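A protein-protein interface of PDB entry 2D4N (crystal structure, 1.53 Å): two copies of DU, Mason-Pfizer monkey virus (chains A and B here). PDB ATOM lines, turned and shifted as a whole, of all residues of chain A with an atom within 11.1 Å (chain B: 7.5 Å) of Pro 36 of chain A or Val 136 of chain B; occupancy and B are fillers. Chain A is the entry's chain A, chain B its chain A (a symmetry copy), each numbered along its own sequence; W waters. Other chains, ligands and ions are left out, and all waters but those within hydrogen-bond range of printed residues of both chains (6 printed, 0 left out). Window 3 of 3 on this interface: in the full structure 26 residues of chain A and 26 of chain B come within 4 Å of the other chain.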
ATOM      1  N   ILE A  28      -0.886  -8.835  21.534  1.00  0.00           N
ATOM      2  CA  ILE A  28      -0.126  -7.788  22.240  1.00  0.00           C
ATOM      3  C   ILE A  28      -0.962  -6.887  23.123  1.00  0.00           C
ATOM      4  O   ILE A  28      -0.406  -6.306  24.047  1.00  0.00           O
ATOM      5  CB  ILE A  28       0.868  -6.955  21.374  1.00  0.00           C
ATOM      6  CG1 ILE A  28       0.132  -6.051  20.449  1.00  0.00           C
ATOM      7  CG2 ILE A  28       1.945  -7.859  20.653  1.00  0.00           C
ATOM      8  CD1 ILE A  28       0.893  -4.787  20.292  1.00  0.00           C
ATOM      9  N   SER A  29      -2.288  -6.829  22.887  1.00  0.00           N
ATOM     10  CA  SER A  29      -3.186  -6.028  23.736  1.00  0.00           C
ATOM     11  C   SER A  29      -3.150  -6.510  25.198  1.00  0.00           C
ATOM     12  O   SER A  29      -3.653  -5.807  26.088  1.00  0.00           O
ATOM     13  CB  SER A  29      -4.623  -6.040  23.163  1.00  0.00           C
ATOM     14  OG  SER A  29      -5.165  -7.351  23.130  1.00  0.00           O
ATOM     15  N   LYS A  30      -2.678  -7.727  25.436  1.00  0.00           N
ATOM     16  CA  LYS A  30      -2.633  -8.304  26.805  1.00  0.00           C
ATOM     17  C   LYS A  30      -1.435  -7.861  27.602  1.00  0.00           C
ATOM     18  O   LYS A  30      -1.392  -8.067  28.813  1.00  0.00           O
ATOM     19  CB  LYS A  30      -2.675  -9.849  26.772  1.00  0.00           C
ATOM     20  CG  LYS A  30      -4.005 -10.412  26.248  1.00  0.00           C
ATOM     21  CD  LYS A  30      -5.211 -10.072  27.138  1.00  0.00           C
ATOM     22  CE  LYS A  30      -6.533 -10.346  26.433  1.00  0.00           C
ATOM     23  NZ  LYS A  30      -6.651 -11.767  25.988  1.00  0.00           N
ATOM     24  N   LEU A  31      -0.450  -7.261  26.930  1.00  0.00           N
ATOM     25  CA  LEU A  31       0.767  -6.807  27.641  1.00  0.00           C
ATOM     26  C   LEU A  31       0.440  -5.596  28.482  1.00  0.00           C
ATOM     27  O   LEU A  31      -0.512  -4.867  28.190  1.00  0.00           O
ATOM     28  CB  LEU A  31       1.872  -6.410  26.639  1.00  0.00           C
ATOM     29  CG  LEU A  31       2.261  -7.556  25.685  1.00  0.00           C
ATOM     30  CD1 LEU A  31       3.333  -7.067  24.709  1.00  0.00           C
ATOM     31  CD2 LEU A  31       2.825  -8.696  26.530  1.00  0.00           C
ATOM     32  N   THR A  32       1.245  -5.384  29.523  1.00  0.00           N
ATOM     33  CA  THR A  32       1.058  -4.221  30.414  1.00  0.00           C
ATOM     34  C   THR A  32       2.290  -3.332  30.428  1.00  0.00           C
ATOM     35  O   THR A  32       3.366  -3.772  30.049  1.00  0.00           O
ATOM     36  CB  THR A  32       0.745  -4.639  31.873  1.00  0.00           C
ATOM     37  OG1 THR A  32       1.829  -5.413  32.372  1.00  0.00           O
ATOM     38  CG2 THR A  32      -0.530  -5.454  31.926  1.00  0.00           C
ATOM     39  N   ARG A  33       2.086  -2.076  30.835  1.00  0.00           N
ATOM     40  CA  ARG A  33       3.152  -1.094  31.048  1.00  0.00           C
ATOM     41  C   ARG A  33       3.443  -1.047  32.538  1.00  0.00           C
ATOM     42  O   ARG A  33       2.552  -1.294  33.370  1.00  0.00           O
ATOM     43  CB  ARG A  33       2.678   0.318  30.645  1.00  0.00           C
ATOM     44  CG  ARG A  33       2.544   0.511  29.152  1.00  0.00           C
ATOM     45  CD  ARG A  33       2.278   1.966  28.759  1.00  0.00           C
ATOM     46  NE  ARG A  33       1.781   1.910  27.390  1.00  0.00           N
ATOM     47  CZ  ARG A  33       2.539   1.803  26.297  1.00  0.00           C
ATOM     48  NH1 ARG A  33       3.863   1.881  26.369  1.00  0.00           N
ATOM     49  NH2 ARG A  33       1.931   1.628  25.115  1.00  0.00           N
ATOM     50  N   ALA A  34       4.665  -0.682  32.907  1.00  0.00           N
ATOM     51  CA  ALA A  34       5.002  -0.597  34.347  1.00  0.00           C
ATOM     52  C   ALA A  34       4.254   0.594  34.997  1.00  0.00           C
ATOM     53  O   ALA A  34       3.759   0.524  36.146  1.00  0.00           O
ATOM     54  CB  ALA A  34       6.512  -0.471  34.515  1.00  0.00           C
ATOM     55  N   THR A  35       4.142   1.663  34.217  1.00  0.00           N
ATOM     56  CA  THR A  35       3.566   2.930  34.645  1.00  0.00           C
ATOM     57  C   THR A  35       2.949   3.534  33.421  1.00  0.00           C
ATOM     58  O   THR A  35       3.347   3.206  32.311  1.00  0.00           O
ATOM     59  CB  THR A  35       4.667   3.924  35.161  1.00  0.00           C
ATOM     60  OG1 THR A  35       5.479   4.373  34.064  1.00  0.00           O
ATOM     61  CG2 THR A  35       5.534   3.299  36.244  1.00  0.00           C
ATOM     62  N   PRO A  36       2.026   4.489  33.582  1.00  0.00           N
ATOM     63  CA  PRO A  36       1.397   5.123  32.410  1.00  0.00           C
ATOM     64  C   PRO A  36       2.407   5.750  31.427  1.00  0.00           C
ATOM     65  O   PRO A  36       2.195   5.709  30.200  1.00  0.00           O
ATOM     66  CB  PRO A  36       0.448   6.188  33.018  1.00  0.00           C
ATOM     67  CG  PRO A  36       0.288   5.809  34.464  1.00  0.00           C
ATOM     68  CD  PRO A  36       1.494   4.996  34.871  1.00  0.00           C
ATOM     69  N   GLY A  37       3.522   6.258  31.950  1.00  0.00           N
ATOM     70  CA  GLY A  37       4.544   6.862  31.100  1.00  0.00           C
ATOM     71  C   GLY A  37       5.649   5.925  30.598  1.00  0.00           C
ATOM     72  O   GLY A  37       6.562   6.394  29.908  1.00  0.00           O
ATOM     73  N   SER A  38       5.536   4.621  30.915  1.00  0.00           N
ATOM     74  CA  SER A  38       6.552   3.633  30.427  1.00  0.00           C
ATOM     75  C   SER A  38       6.491   3.488  28.907  1.00  0.00           C
ATOM     76  O   SER A  38       5.425   3.325  28.354  1.00  0.00           O
ATOM     77  CB  SER A  38       6.373   2.282  31.146  1.00  0.00           C
ATOM     78  OG  SER A  38       6.664   2.414  32.545  1.00  0.00           O
ATOM     79  N   ALA A  39       7.615   3.584  28.206  1.00  0.00           N
ATOM     80  CA  ALA A  39       7.617   3.431  26.737  1.00  0.00           C
ATOM     81  C   ALA A  39       7.345   1.953  26.346  1.00  0.00           C
ATOM     82  O   ALA A  39       6.743   1.688  25.297  1.00  0.00           O
ATOM     83  CB  ALA A  39       8.933   3.893  26.125  1.00  0.00           C
ATOM     84  N   GLY A  40       7.839   1.000  27.153  1.00  0.00           N
ATOM     85  CA  GLY A  40       7.787  -0.409  26.726  1.00  0.00           C
ATOM     86  C   GLY A  40       6.631  -1.177  27.347  1.00  0.00           C
ATOM     87  O   GLY A  40       6.090  -0.829  28.415  1.00  0.00           O
ATOM     88  N   LEU A  41       6.252  -2.209  26.582  1.00  0.00           N
ATOM     89  CA  LEU A  41       5.222  -3.175  27.041  1.00  0.00           C
ATOM     90  C   LEU A  41       6.017  -4.388  27.506  1.00  0.00           C
ATOM     91  O   LEU A  41       6.743  -4.971  26.722  1.00  0.00           O
ATOM     92  CB  LEU A  41       4.351  -3.533  25.844  1.00  0.00           C
ATOM     93  CG  LEU A  41       3.509  -2.342  25.374  1.00  0.00           C
ATOM     94  CD1 LEU A  41       2.757  -2.762  24.073  1.00  0.00           C
ATOM     95  CD2 LEU A  41       2.526  -1.914  26.442  1.00  0.00           C
ATOM     96  N   ASP A  42       5.853  -4.795  28.746  1.00  0.00           N
ATOM     97  CA  ASP A  42       6.778  -5.809  29.265  1.00  0.00           C
ATOM     98  C   ASP A  42       6.423  -7.204  28.756  1.00  0.00           C
ATOM     99  O   ASP A  42       5.240  -7.559  28.609  1.00  0.00           O
ATOM    100  CB  ASP A  42       6.820  -5.744  30.784  1.00  0.00           C
ATOM    101  CG  ASP A  42       7.514  -4.476  31.244  1.00  0.00           C
ATOM    102  OD1 ASP A  42       8.510  -4.067  30.605  1.00  0.00           O
ATOM    103  OD2 ASP A  42       7.074  -3.920  32.253  1.00  0.00           O
ATOM    104  N   ARG A 120       9.534 -10.613  34.186  1.00  0.00           N
ATOM    105  CA  ARG A 120       9.588  -9.730  33.032  1.00  0.00           C
ATOM    106  C   ARG A 120      11.023  -9.602  32.580  1.00  0.00           C
ATOM    107  O   ARG A 120      11.873  -9.181  33.344  1.00  0.00           O
ATOM    108  CB  ARG A 120       9.022  -8.353  33.373  1.00  0.00           C
ATOM    109  CG  ARG A 120       7.500  -8.409  33.663  1.00  0.00           C
ATOM    110  CD  ARG A 120       7.005  -7.116  34.363  1.00  0.00           C
ATOM    111  NE  ARG A 120       7.635  -6.942  35.671  1.00  0.00           N
ATOM    112  CZ  ARG A 120       7.894  -5.764  36.235  1.00  0.00           C
ATOM    113  NH1 ARG A 120       7.578  -4.647  35.600  1.00  0.00           N
ATOM    114  NH2 ARG A 120       8.458  -5.703  37.449  1.00  0.00           N
ATOM    115  N   ASN B  96       9.288   8.590  28.859  1.00  0.00           N
ATOM    116  CA  ASN B  96       8.982  10.029  28.714  1.00  0.00           C
ATOM    117  C   ASN B  96       9.058  10.818  30.007  1.00  0.00           C
ATOM    118  O   ASN B  96       9.600  11.976  30.051  1.00  0.00           O
ATOM    119  CB  ASN B  96       7.572  10.226  28.133  1.00  0.00           C
ATOM    120  CG  ASN B  96       7.220  11.730  28.057  1.00  0.00           C
ATOM    121  OD1 ASN B  96       6.522  12.253  28.941  1.00  0.00           O
ATOM    122  ND2 ASN B  96       7.774  12.422  27.066  1.00  0.00           N
ATOM    123  N   ASP B  97       8.528  10.208  31.058  1.00  0.00           N
ATOM    124  CA  ASP B  97       8.448  10.932  32.334  1.00  0.00           C
ATOM    125  C   ASP B  97       9.479  10.498  33.365  1.00  0.00           C
ATOM    126  O   ASP B  97       9.301  10.778  34.559  1.00  0.00           O
ATOM    127  CB  ASP B  97       7.014  10.881  32.872  1.00  0.00           C
ATOM    128  CG  ASP B  97       6.541   9.468  33.129  1.00  0.00           C
ATOM    129  OD1 ASP B  97       7.263   8.479  32.836  1.00  0.00           O
ATOM    130  OD2 ASP B  97       5.422   9.366  33.671  1.00  0.00           O
ATOM    131  N   LEU B 129       6.374   8.715  20.960  1.00  0.00           N
ATOM    132  CA  LEU B 129       5.769   7.771  21.874  1.00  0.00           C
ATOM    133  C   LEU B 129       4.356   7.470  21.403  1.00  0.00           C
ATOM    134  O   LEU B 129       3.501   8.362  21.389  1.00  0.00           O
ATOM    135  CB  LEU B 129       5.785   8.375  23.276  1.00  0.00           C
ATOM    136  CG  LEU B 129       5.142   7.540  24.406  1.00  0.00           C
ATOM    137  CD1 LEU B 129       5.835   6.178  24.606  1.00  0.00           C
ATOM    138  CD2 LEU B 129       5.203   8.352  25.740  1.00  0.00           C
ATOM    139  N   ASP B 133      -4.030   1.288  24.302  1.00  0.00           N
ATOM    140  CA  ASP B 133      -4.930   1.013  25.418  1.00  0.00           C
ATOM    141  C   ASP B 133      -4.389  -0.041  26.396  1.00  0.00           C
ATOM    142  O   ASP B 133      -5.124  -0.510  27.287  1.00  0.00           O
ATOM    143  CB  ASP B 133      -6.293   0.555  24.885  1.00  0.00           C
ATOM    144  CG  ASP B 133      -6.995   1.624  24.042  1.00  0.00           C
ATOM    145  OD1 ASP B 133      -7.689   1.243  23.070  1.00  0.00           O
ATOM    146  OD2 ASP B 133      -6.872   2.835  24.352  1.00  0.00           O
ATOM    147  N   ASN B 134      -3.105  -0.439  26.274  1.00  0.00           N
ATOM    148  CA  ASN B 134      -2.614  -1.456  27.193  1.00  0.00           C
ATOM    149  C   ASN B 134      -2.705  -0.962  28.630  1.00  0.00           C
ATOM    150  O   ASN B 134      -2.459   0.225  28.912  1.00  0.00           O
ATOM    151  CB  ASN B 134      -1.154  -1.823  26.935  1.00  0.00           C
ATOM    152  CG  ASN B 134      -0.941  -2.569  25.597  1.00  0.00           C
ATOM    153  OD1 ASN B 134      -0.853  -3.812  25.559  1.00  0.00           O
ATOM    154  ND2 ASN B 134      -0.913  -1.819  24.530  1.00  0.00           N
ATOM    155  N   LYS B 135      -3.028  -1.876  29.526  1.00  0.00           N
ATOM    156  CA  LYS B 135      -3.211  -1.528  30.912  1.00  0.00           C
ATOM    157  C   LYS B 135      -1.874  -1.385  31.625  1.00  0.00           C
ATOM    158  O   LYS B 135      -0.813  -1.799  31.117  1.00  0.00           O
ATOM    159  CB  LYS B 135      -4.089  -2.593  31.572  1.00  0.00           C
ATOM    160  CG  LYS B 135      -5.579  -2.448  31.190  1.00  0.00           C
ATOM    161  CD  LYS B 135      -6.376  -3.708  31.535  1.00  0.00           C
ATOM    162  N   VAL B 136      -1.926  -0.766  32.801  1.00  0.00           N
ATOM    163  CA  VAL B 136      -0.770  -0.623  33.685  1.00  0.00           C
ATOM    164  C   VAL B 136      -0.691  -1.799  34.682  1.00  0.00           C
ATOM    165  O   VAL B 136      -1.725  -2.274  35.168  1.00  0.00           O
ATOM    166  CB  VAL B 136      -0.809   0.735  34.399  1.00  0.00           C
ATOM    167  CG1 VAL B 136       0.305   0.845  35.409  1.00  0.00           C
ATOM    168  CG2 VAL B 136      -0.719   1.860  33.388  1.00  0.00           C
ATOM    169  N   GLN B 137       0.521  -2.282  34.964  1.00  0.00           N
ATOM    170  CA  GLN B 137       0.731  -3.471  35.823  1.00  0.00           C
ATOM    171  C   GLN B 137       0.040  -3.366  37.191  1.00  0.00           C
ATOM    172  O   GLN B 137       0.004  -2.286  37.804  1.00  0.00           O
ATOM    173  CB  GLN B 137       2.228  -3.754  36.002  1.00  0.00           C
ATOM    174  CG  GLN B 137       2.937  -2.853  37.042  1.00  0.00           C
HETATM  175  O   HOH W   1      -4.744  -2.963  25.139  1.00  0.00           O
HETATM  176  O   HOH W   2      -0.976   2.113  27.616  1.00  0.00           O
HETATM  177  O   HOH W   3       7.418   6.184  34.041  1.00  0.00           O
HETATM  178  O   HOH W   4       3.907   7.336  34.622  1.00  0.00           O
HETATM  179  O   HOH W   5      -3.186  -4.619  28.881  1.00  0.00           O
HETATM  180  O   HOH W   6       7.483   6.836  27.572  1.00  0.00           O
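The side-chain amide oxygen (OD1) of Asn 134 of chain B lies close to the backbone carbonyl oxygen (O) of Ile 28 of chain A (3.0 Å). O of Ser 29 of chain A lies close to OD1 of Asn 134 of chain B. The backbone carbonyl oxygen of Leu 31 of chain A lies close to the side-chain amide oxygen of Asn 134 of chain B (2.9 Å). The backbone carbonyl oxygen (O) of Lys 135 of chain B sits at hydrogen-bond distance from the backbone NH (N) of Arg 33 of chain A, at 2.9 Å. The backbone NH (N) of Gln 137 of chain B sits at hydrogen-bond distance from the backbone carbonyl oxygen (O) of Arg 33 of chain A, at 2.8 Å.
The backbone carbonyl oxygen (O) of Thr 32 of chain A lies within hydrogen-bond range of the backbone NH (N) of Asp 42 of chain A (3.0 Å). NH1 of Arg 33 of chain A sits at hydrogen-bond distance from O of Ser 38 of chain A, 2.9 Å away. O of Ala 39 of chain A sits at hydrogen-bond distance from NH1 of Arg 33 of chain A, at 3.1 Å. N of Gly 37 of chain A sits close to OG1 of Thr 35 of chain A, at 3.4 Å. OG1 of Thr 35 of chain A lies within hydrogen-bond range of OG of Ser 38 of chain A (2.7 Å).
Among the printed residues, merely in contact across the chains: Thr 32 of chain A with Lys 135 of chain B (3.1 Å), Arg 33 of chain A with Val 136 of chain B (3.4 Å), Ala 34 of chain A with Val 136 of chain B (3.5 Å), Ala 34 of chain A with Gln 137 of chain B (3.6 Å), Gly 37 of chain A with Asp 97 of chain B (3.6 Å), Leu 41 of chain A with Asn 134 of chain B (3.6 Å), Gly 37 of chain A with Asn 96 of chain B (3.7 Å), Pro 36 of chain A with Val 136 of chain B (3.8 Å), Thr 32 of chain A with Gln 137 of chain B (3.9 Å), Ala 39 of chain A with Leu 129 of chain B (3.9 Å) and Thr 35 of chain A with Val 136 of chain B (3.9 Å).
Of the printed residues of chain B, Ile 28 of chain A touches Asn 134 (3.0 Å). Pro 36 of chain A touches just one residue of chain B: Val 136 (3.8 Å). Of the printed residues of chain B, Gly 37 of chain A touches Asn 96 and Asp 97. Of the printed residues of chain B, Ala 39 of chain A touches Leu 129 (3.9 Å). Printed residues of chain A within 4 Å of Asn 96 of chain B: Gly 37 (3.7 Å). Printed residues of chain A within 4 Å of Asn 134 of chain B: Ile 28, Ser 29, Leu 31 and Leu 41. Val 136 of chain B touches four residues of chain A. Of chain A, only Thr 32 (3.9 Å), Arg 33 (2.8 Å) and Ala 34 (3.6 Å) come within 4 Å of Gln 137 of chain B. The nearest residue of chain B that does not touch Pro 36 of chain A is Asp 97 of chain B (5.2 Å). The nearest residue of chain A that does not touch Val 136 of chain B is Thr 32 of chain A (4.2 Å).
Printed residues of chain B that touch a printed residue of chain A: Asn 96, Asp 97, Leu 129, Asn 134, Lys 135, Val 136 and Gln 137. Of the 16 printed residues of chain A, 11 touch a printed residue of chain B. Among the printed residues, 16 pairs touch across the chains.
No position is printed for both chains. Of the 16 pairs that touch across the chains among the printed residues, none has its exchanged pair printed and touching as well.
Water W6 lies within hydrogen-bond range of the backbone carbonyl oxygen of Gly 37 of chain A (2.5 Å), the backbone NH of Asn 96 of chain B (2.8 Å) and the backbone NH of Ala 39 of chain A (3.3 Å). Water W3 lies within hydrogen-bond range of the side-chain carboxylate of Asp 97 of chain B (2.6 Å) and the side-chain hydroxyl of Thr 35 of chain A (2.7 Å). Water W4 lies within hydrogen-bond range of OD2 of Asp 97 of chain B (2.7 Å), N of Gly 37 of chain A (2.9 Å) and OG1 of Thr 35 of chain A (3.4 Å). Water W2 lies within hydrogen-bond range of the backbone carbonyl oxygen (O) of Asn 134 of chain B and the guanidinium group (NE) of Arg 33 of chain A. Water W5 lies within hydrogen-bond range of the backbone carbonyl oxygen (O) of Leu 31 of chain A, the backbone NH (N) of Lys 135 of chain B and the backbone carbonyl oxygen (O) of Ser 29 of chain A. Water W1 lies within hydrogen-bond range of the backbone carbonyl oxygen of Ser 29 of chain A, the backbone NH of Asn 134 of chain B and the backbone carbonyl oxygen of Asp 133 of chain B.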
